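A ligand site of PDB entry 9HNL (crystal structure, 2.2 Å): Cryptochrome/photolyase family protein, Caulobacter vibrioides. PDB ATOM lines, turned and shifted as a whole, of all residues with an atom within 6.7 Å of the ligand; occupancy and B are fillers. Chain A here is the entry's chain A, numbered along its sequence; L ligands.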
ATOM      1  N   ASP A 346      -7.105 -29.751 -17.432  1.00  0.00           N
ATOM      2  CA  ASP A 346      -5.683 -30.085 -17.521  1.00  0.00           C
ATOM      3  C   ASP A 346      -4.810 -29.139 -16.721  1.00  0.00           C
ATOM      4  O   ASP A 346      -3.585 -29.314 -16.694  1.00  0.00           O
ATOM      5  CB  ASP A 346      -5.241 -30.093 -18.985  1.00  0.00           C
ATOM      6  CG  ASP A 346      -5.547 -31.414 -19.668  1.00  0.00           C
ATOM      7  OD1 ASP A 346      -5.852 -32.406 -18.964  1.00  0.00           O
ATOM      8  OD2 ASP A 346      -5.471 -31.467 -20.918  1.00  0.00           O
ATOM      9  N   MET A 347      -5.385 -28.132 -16.060  1.00  0.00           N
ATOM     10  CA  MET A 347      -4.634 -27.254 -15.176  1.00  0.00           C
ATOM     11  C   MET A 347      -4.469 -27.976 -13.840  1.00  0.00           C
ATOM     12  O   MET A 347      -5.440 -28.133 -13.091  1.00  0.00           O
ATOM     13  CB  MET A 347      -5.357 -25.926 -14.966  1.00  0.00           C
ATOM     14  CG  MET A 347      -5.926 -25.289 -16.216  1.00  0.00           C
ATOM     15  SD  MET A 347      -5.929 -23.505 -16.040  1.00  0.00           S
ATOM     16  CE  MET A 347      -7.625 -23.137 -16.448  1.00  0.00           C
ATOM     17  N   ALA A 348      -3.241 -28.409 -13.541  1.00  0.00           N
ATOM     18  CA  ALA A 348      -3.004 -29.178 -12.329  1.00  0.00           C
ATOM     19  C   ALA A 348      -3.355 -28.380 -11.073  1.00  0.00           C
ATOM     20  O   ALA A 348      -3.945 -28.912 -10.136  1.00  0.00           O
ATOM     21  CB  ALA A 348      -1.546 -29.647 -12.275  1.00  0.00           C
ATOM     22  N   CYS A 349      -3.008 -27.093 -11.054  1.00  0.00           N
ATOM     23  CA  CYS A 349      -3.279 -26.262  -9.884  1.00  0.00           C
ATOM     24  C   CYS A 349      -4.780 -26.137  -9.630  1.00  0.00           C
ATOM     25  O   CYS A 349      -5.245 -26.283  -8.495  1.00  0.00           O
ATOM     26  CB  CYS A 349      -2.639 -24.884 -10.056  1.00  0.00           C
ATOM     27  SG  CYS A 349      -3.091 -24.062 -11.608  1.00  0.00           S
ATOM     28  N   VAL A 350      -5.548 -25.863 -10.680  1.00  0.00           N
ATOM     29  CA  VAL A 350      -6.993 -25.732 -10.526  1.00  0.00           C
ATOM     30  C   VAL A 350      -7.617 -27.073 -10.192  1.00  0.00           C
ATOM     31  O   VAL A 350      -8.508 -27.171  -9.343  1.00  0.00           O
ATOM     32  CB  VAL A 350      -7.612 -25.116 -11.805  1.00  0.00           C
ATOM     33  CG1 VAL A 350      -9.123 -25.023 -11.670  1.00  0.00           C
ATOM     34  CG2 VAL A 350      -7.010 -23.750 -12.080  1.00  0.00           C
ATOM     35  N   VAL A 371      -5.363 -19.206  -7.043  1.00  0.00           N
ATOM     36  CA  VAL A 371      -5.621 -20.229  -8.062  1.00  0.00           C
ATOM     37  C   VAL A 371      -7.016 -20.040  -8.641  1.00  0.00           C
ATOM     38  O   VAL A 371      -7.161 -19.497  -9.750  1.00  0.00           O
ATOM     39  CB  VAL A 371      -5.445 -21.648  -7.491  1.00  0.00           C
ATOM     40  CG1 VAL A 371      -5.659 -22.683  -8.588  1.00  0.00           C
ATOM     41  CG2 VAL A 371      -4.061 -21.807  -6.869  1.00  0.00           C
ATOM     42  N   SER A 426       0.125 -14.242 -13.110  1.00  0.00           N
ATOM     43  CA  SER A 426       0.273 -15.217 -14.191  1.00  0.00           C
ATOM     44  C   SER A 426       0.615 -16.576 -13.591  1.00  0.00           C
ATOM     45  O   SER A 426       0.582 -16.782 -12.370  1.00  0.00           O
ATOM     46  CB  SER A 426       1.332 -14.746 -15.181  1.00  0.00           C
ATOM     47  OG  SER A 426       2.610 -14.751 -14.589  1.00  0.00           O
ATOM     48  N   GLY A 427       0.973 -17.539 -14.447  1.00  0.00           N
ATOM     49  CA  GLY A 427       1.441 -18.814 -13.959  1.00  0.00           C
ATOM     50  C   GLY A 427       2.780 -18.747 -13.260  1.00  0.00           C
ATOM     51  O   GLY A 427       3.153 -19.691 -12.547  1.00  0.00           O
ATOM     52  N   ALA A 428       3.511 -17.648 -13.438  1.00  0.00           N
ATOM     53  CA  ALA A 428       4.813 -17.499 -12.779  1.00  0.00           C
ATOM     54  C   ALA A 428       4.663 -17.534 -11.262  1.00  0.00           C
ATOM     55  O   ALA A 428       5.495 -18.134 -10.568  1.00  0.00           O
ATOM     56  CB  ALA A 428       5.471 -16.199 -13.222  1.00  0.00           C
ATOM     57  N   ILE A 430       2.197 -19.062  -9.427  1.00  0.00           N
ATOM     58  CA  ILE A 430       1.894 -20.433  -9.014  1.00  0.00           C
ATOM     59  C   ILE A 430       3.130 -21.309  -9.155  1.00  0.00           C
ATOM     60  O   ILE A 430       3.335 -22.231  -8.350  1.00  0.00           O
ATOM     61  CB  ILE A 430       0.707 -20.982  -9.839  1.00  0.00           C
ATOM     62  CG1 ILE A 430      -0.555 -20.168  -9.540  1.00  0.00           C
ATOM     63  CG2 ILE A 430       0.473 -22.448  -9.534  1.00  0.00           C
ATOM     64  CD1 ILE A 430      -1.488 -20.049 -10.720  1.00  0.00           C
ATOM     65  N   ASP A 431       3.970 -21.037 -10.152  1.00  0.00           N
ATOM     66  CA  ASP A 431       5.191 -21.826 -10.328  1.00  0.00           C
ATOM     67  C   ASP A 431       6.154 -21.597  -9.175  1.00  0.00           C
ATOM     68  O   ASP A 431       6.709 -22.556  -8.628  1.00  0.00           O
ATOM     69  CB  ASP A 431       5.847 -21.481 -11.662  1.00  0.00           C
ATOM     70  CG  ASP A 431       6.959 -22.438 -12.027  1.00  0.00           C
ATOM     71  OD1 ASP A 431       6.867 -23.619 -11.629  1.00  0.00           O
ATOM     72  OD2 ASP A 431       7.906 -22.013 -12.706  1.00  0.00           O
ATOM     73  N   SER A 434       4.517 -23.299  -5.737  1.00  0.00           N
ATOM     74  CA  SER A 434       3.952 -24.633  -5.663  1.00  0.00           C
ATOM     75  C   SER A 434       4.822 -25.633  -6.410  1.00  0.00           C
ATOM     76  O   SER A 434       5.805 -25.269  -7.054  1.00  0.00           O
ATOM     77  CB  SER A 434       2.523 -24.661  -6.226  1.00  0.00           C
ATOM     78  OG  SER A 434       2.550 -24.697  -7.639  1.00  0.00           O
ATOM     79  N   TYR A 436       3.252 -27.640  -8.685  1.00  0.00           N
ATOM     80  CA  TYR A 436       2.227 -28.025  -9.640  1.00  0.00           C
ATOM     81  C   TYR A 436       2.740 -28.071 -11.074  1.00  0.00           C
ATOM     82  O   TYR A 436       2.373 -28.979 -11.828  1.00  0.00           O
ATOM     83  CB  TYR A 436       1.050 -27.051  -9.573  1.00  0.00           C
ATOM     84  CG  TYR A 436       0.113 -27.220  -8.395  1.00  0.00           C
ATOM     85  CD1 TYR A 436      -0.381 -28.469  -8.041  1.00  0.00           C
ATOM     86  CD2 TYR A 436      -0.307 -26.123  -7.661  1.00  0.00           C
ATOM     87  CE1 TYR A 436      -1.244 -28.624  -6.972  1.00  0.00           C
ATOM     88  CE2 TYR A 436      -1.164 -26.267  -6.585  1.00  0.00           C
ATOM     89  CZ  TYR A 436      -1.637 -27.518  -6.243  1.00  0.00           C
ATOM     90  OH  TYR A 436      -2.497 -27.660  -5.181  1.00  0.00           O
ATOM     91  N   CYS A 437       3.566 -27.103 -11.458  1.00  0.00           N
ATOM     92  CA  CYS A 437       3.755 -26.808 -12.871  1.00  0.00           C
ATOM     93  C   CYS A 437       4.591 -27.869 -13.589  1.00  0.00           C
ATOM     94  O   CYS A 437       4.359 -28.132 -14.770  1.00  0.00           O
ATOM     95  CB  CYS A 437       4.378 -25.426 -13.039  1.00  0.00           C
ATOM     96  SG  CYS A 437       3.332 -24.076 -12.447  1.00  0.00           S
ATOM     97  N   LYS A 438       5.567 -28.472 -12.906  1.00  0.00           N
ATOM     98  CA  LYS A 438       6.362 -29.502 -13.575  1.00  0.00           C
ATOM     99  C   LYS A 438       5.542 -30.749 -13.864  1.00  0.00           C
ATOM    100  O   LYS A 438       5.789 -31.429 -14.862  1.00  0.00           O
ATOM    101  CB  LYS A 438       7.601 -29.864 -12.765  1.00  0.00           C
ATOM    102  CG  LYS A 438       8.648 -28.750 -12.624  1.00  0.00           C
ATOM    103  CD  LYS A 438       8.235 -27.604 -11.703  1.00  0.00           C
ATOM    104  CE  LYS A 438       9.056 -26.338 -11.981  1.00  0.00           C
ATOM    105  NZ  LYS A 438       8.845 -25.805 -13.361  1.00  0.00           N
ATOM    106  N   GLY A 439       4.563 -31.046 -13.015  1.00  0.00           N
ATOM    107  CA  GLY A 439       3.648 -32.132 -13.298  1.00  0.00           C
ATOM    108  C   GLY A 439       2.486 -31.770 -14.198  1.00  0.00           C
ATOM    109  O   GLY A 439       1.697 -32.649 -14.555  1.00  0.00           O
ATOM    110  N   CYS A 440       2.347 -30.500 -14.555  1.00  0.00           N
ATOM    111  CA  CYS A 440       1.246 -30.038 -15.375  1.00  0.00           C
ATOM    112  C   CYS A 440       1.497 -30.309 -16.854  1.00  0.00           C
ATOM    113  O   CYS A 440       2.646 -30.293 -17.310  1.00  0.00           O
ATOM    114  CB  CYS A 440       1.005 -28.544 -15.155  1.00  0.00           C
ATOM    115  SG  CYS A 440      -0.479 -27.877 -15.958  1.00  0.00           S
ATOM    116  N   ARG A 441       0.418 -30.563 -17.590  1.00  0.00           N
ATOM    117  CA  ARG A 441       0.539 -30.775 -19.040  1.00  0.00           C
ATOM    118  C   ARG A 441       0.900 -29.483 -19.760  1.00  0.00           C
ATOM    119  O   ARG A 441       1.528 -29.522 -20.832  1.00  0.00           O
ATOM    120  CB  ARG A 441      -0.757 -31.388 -19.571  1.00  0.00           C
ATOM    121  CG  ARG A 441      -1.148 -31.062 -21.011  1.00  0.00           C
ATOM    122  CD  ARG A 441      -2.138 -29.898 -21.099  1.00  0.00           C
ATOM    123  NE  ARG A 441      -2.712 -29.750 -22.428  1.00  0.00           N
ATOM    124  CZ  ARG A 441      -2.030 -29.517 -23.541  1.00  0.00           C
ATOM    125  NH1 ARG A 441      -0.714 -29.381 -23.530  1.00  0.00           N
ATOM    126  NH2 ARG A 441      -2.681 -29.430 -24.692  1.00  0.00           N
ATOM    127  N   TYR A 442       0.550 -28.342 -19.190  1.00  0.00           N
ATOM    128  CA  TYR A 442       0.874 -27.063 -19.802  1.00  0.00           C
ATOM    129  C   TYR A 442       2.315 -26.673 -19.470  1.00  0.00           C
ATOM    130  O   TYR A 442       2.953 -27.228 -18.567  1.00  0.00           O
ATOM    131  CB  TYR A 442      -0.093 -25.986 -19.322  1.00  0.00           C
ATOM    132  CG  TYR A 442      -1.519 -26.205 -19.787  1.00  0.00           C
ATOM    133  CD1 TYR A 442      -1.866 -26.035 -21.126  1.00  0.00           C
ATOM    134  CD2 TYR A 442      -2.518 -26.572 -18.892  1.00  0.00           C
ATOM    135  CE1 TYR A 442      -3.164 -26.231 -21.551  1.00  0.00           C
ATOM    136  CE2 TYR A 442      -3.819 -26.759 -19.314  1.00  0.00           C
ATOM    137  CZ  TYR A 442      -4.139 -26.594 -20.638  1.00  0.00           C
ATOM    138  OH  TYR A 442      -5.432 -26.786 -21.071  1.00  0.00           O
ATOM    139  N   ASP A 443       2.823 -25.701 -20.229  1.00  0.00           N
ATOM    140  CA  ASP A 443       4.171 -25.171 -20.049  1.00  0.00           C
ATOM    141  C   ASP A 443       4.046 -23.765 -19.479  1.00  0.00           C
ATOM    142  O   ASP A 443       3.602 -22.847 -20.172  1.00  0.00           O
ATOM    143  CB  ASP A 443       4.925 -25.159 -21.382  1.00  0.00           C
ATOM    144  CG  ASP A 443       6.406 -24.852 -21.210  1.00  0.00           C
ATOM    145  OD1 ASP A 443       6.798 -24.330 -20.147  1.00  0.00           O
ATOM    146  OD2 ASP A 443       7.180 -25.150 -22.143  1.00  0.00           O
ATOM    147  N   VAL A 444       4.450 -23.601 -18.218  1.00  0.00           N
ATOM    148  CA  VAL A 444       4.334 -22.319 -17.542  1.00  0.00           C
ATOM    149  C   VAL A 444       5.284 -21.267 -18.088  1.00  0.00           C
ATOM    150  O   VAL A 444       5.131 -20.075 -17.774  1.00  0.00           O
ATOM    151  CB  VAL A 444       4.554 -22.492 -16.021  1.00  0.00           C
ATOM    152  CG1 VAL A 444       6.030 -22.426 -15.675  1.00  0.00           C
ATOM    153  CG2 VAL A 444       3.753 -21.455 -15.241  1.00  0.00           C
ATOM    154  N   LYS A 445       6.255 -21.653 -18.909  1.00  0.00           N
ATOM    155  CA  LYS A 445       7.182 -20.714 -19.516  1.00  0.00           C
ATOM    156  C   LYS A 445       6.702 -20.208 -20.877  1.00  0.00           C
ATOM    157  O   LYS A 445       7.431 -19.455 -21.523  1.00  0.00           O
ATOM    158  CB  LYS A 445       8.570 -21.338 -19.657  1.00  0.00           C
ATOM    159  CG  LYS A 445       9.268 -21.617 -18.329  1.00  0.00           C
ATOM    160  CD  LYS A 445      10.408 -22.604 -18.500  1.00  0.00           C
ATOM    161  CE  LYS A 445      10.034 -23.747 -19.429  1.00  0.00           C
ATOM    162  NZ  LYS A 445       9.250 -24.807 -18.730  1.00  0.00           N
ATOM    163  N   ALA A 452       0.684 -23.640 -23.880  1.00  0.00           N
ATOM    164  CA  ALA A 452       0.928 -22.525 -22.970  1.00  0.00           C
ATOM    165  C   ALA A 452       0.037 -22.627 -21.735  1.00  0.00           C
ATOM    166  O   ALA A 452      -1.126 -23.017 -21.828  1.00  0.00           O
ATOM    167  CB  ALA A 452       0.675 -21.205 -23.705  1.00  0.00           C
ATOM    168  N   CYS A 453       0.600 -22.281 -20.587  1.00  0.00           N
ATOM    169  CA  CYS A 453      -0.173 -22.204 -19.355  1.00  0.00           C
ATOM    170  C   CYS A 453      -1.259 -21.144 -19.508  1.00  0.00           C
ATOM    171  O   CYS A 453      -0.934 -19.992 -19.809  1.00  0.00           O
ATOM    172  CB  CYS A 453       0.723 -21.884 -18.182  1.00  0.00           C
ATOM    173  SG  CYS A 453      -0.122 -21.266 -16.724  1.00  0.00           S
ATOM    174  N   PRO A 454      -2.550 -21.471 -19.331  1.00  0.00           N
ATOM    175  CA  PRO A 454      -3.599 -20.470 -19.610  1.00  0.00           C
ATOM    176  C   PRO A 454      -3.503 -19.221 -18.752  1.00  0.00           C
ATOM    177  O   PRO A 454      -3.898 -18.154 -19.203  1.00  0.00           O
ATOM    178  CB  PRO A 454      -4.913 -21.226 -19.360  1.00  0.00           C
ATOM    179  CG  PRO A 454      -4.561 -22.633 -19.199  1.00  0.00           C
ATOM    180  CD  PRO A 454      -3.097 -22.812 -19.036  1.00  0.00           C
ATOM    181  N   PHE A 455      -2.950 -19.322 -17.529  1.00  0.00           N
ATOM    182  CA  PHE A 455      -2.837 -18.156 -16.656  1.00  0.00           C
ATOM    183  C   PHE A 455      -1.987 -17.056 -17.284  1.00  0.00           C
ATOM    184  O   PHE A 455      -2.156 -15.881 -16.961  1.00  0.00           O
ATOM    185  CB  PHE A 455      -2.249 -18.562 -15.299  1.00  0.00           C
ATOM    186  CG  PHE A 455      -3.254 -19.137 -14.342  1.00  0.00           C
ATOM    187  CD1 PHE A 455      -3.500 -20.509 -14.307  1.00  0.00           C
ATOM    188  CD2 PHE A 455      -3.937 -18.317 -13.462  1.00  0.00           C
ATOM    189  CE1 PHE A 455      -4.420 -21.032 -13.413  1.00  0.00           C
ATOM    190  CE2 PHE A 455      -4.854 -18.849 -12.570  1.00  0.00           C
ATOM    191  CZ  PHE A 455      -5.098 -20.209 -12.541  1.00  0.00           C
ATOM    192  N   ASN A 456      -1.066 -17.422 -18.178  1.00  0.00           N
ATOM    193  CA  ASN A 456      -0.112 -16.458 -18.708  1.00  0.00           C
ATOM    194  C   ASN A 456      -0.794 -15.453 -19.630  1.00  0.00           C
ATOM    195  O   ASN A 456      -0.723 -14.232 -19.412  1.00  0.00           O
ATOM    196  CB  ASN A 456       1.023 -17.186 -19.427  1.00  0.00           C
ATOM    197  CG  ASN A 456       1.993 -17.827 -18.463  1.00  0.00           C
ATOM    198  OD1 ASN A 456       2.072 -17.440 -17.291  1.00  0.00           O
ATOM    199  ND2 ASN A 456       2.744 -18.813 -18.942  1.00  0.00           N
HETATM  200 FE1  LIG L   1       1.297 -24.256 -13.444  1.00  0.00          FE
HETATM  201 FE2  LIG L   1      -0.242 -23.098 -15.383  1.00  0.00          FE
HETATM  202 FE3  LIG L   1      -1.419 -24.160 -13.144  1.00  0.00          FE
HETATM  203 FE4  LIG L   1      -0.307 -25.814 -15.032  1.00  0.00          FE
HETATM  204  S1  LIG L   1      -2.097 -24.423 -15.307  1.00  0.00           S
HETATM  205  S2  LIG L   1      -0.062 -25.949 -12.767  1.00  0.00           S
HETATM  206  S3  LIG L   1       1.475 -24.552 -15.706  1.00  0.00           S
HETATM  207  S4  LIG L   1       0.013 -22.382 -13.228  1.00  0.00           S
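CB of Met 347 touches S1 of the ligand, at 3.6 Å.
Gly 427 touches the ligand (CA to S4, 3.9 Å).
Ile 430 touches the ligand (CG2 to S4, 3.7 Å).
Tyr 436 touches the ligand (CB to S2, 3.6 Å).
Val 444 touches the ligand.
Hydrophobic or aromatic side chains within 4 Å of the ligand: Met 347, Ile 430, Tyr 436 and Val 444.
The nearest printed residue that does not touch the ligand is Ala 348 (4.01 Å).
The backbone NH of Cys 349 lies close to a sulfur (S2) of the ligand (3.6 Å).
An iron atom (FE4) of the ligand is bound by the side-chain sulfur (SG) of Cys 440 (2.3 Å).
SG of Cys 453 is bound to FE2 of the ligand (2.3 Å).
The side-chain sulfur (SG) of Cys 437 is bound to an iron atom (FE1) of the ligand, 2.3 Å away.
The side-chain sulfur (SG) of Cys 349 binds an iron atom (FE3) of the ligand (2.3 Å).
N of Cys 453 lies within hydrogen-bond range of O of Asp 443 (3.1 Å).
OG of Ser 434 sits close to N of Tyr 436 (3.2 Å).
The side-chain amide nitrogen (ND2) of Asn 456 sits at hydrogen-bond distance from the backbone carbonyl oxygen (O) of Val 444, at 2.9 Å.
N of Ala 348 lies close to SG of Cys 440 (3.7 Å).
The side-chain carboxylate (OD1) of Asp 431 lies close to the side-chain sulfur (SG) of Cys 437.
The side-chain sulfur of Cys 440 lies close to the backbone carbonyl oxygen of Asp 346 (3.5 Å).
OD1 of Asn 456 lies within hydrogen-bond range of N of Gly 427.
SG of Cys 440 sits close to N of Tyr 442 (3.4 Å).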
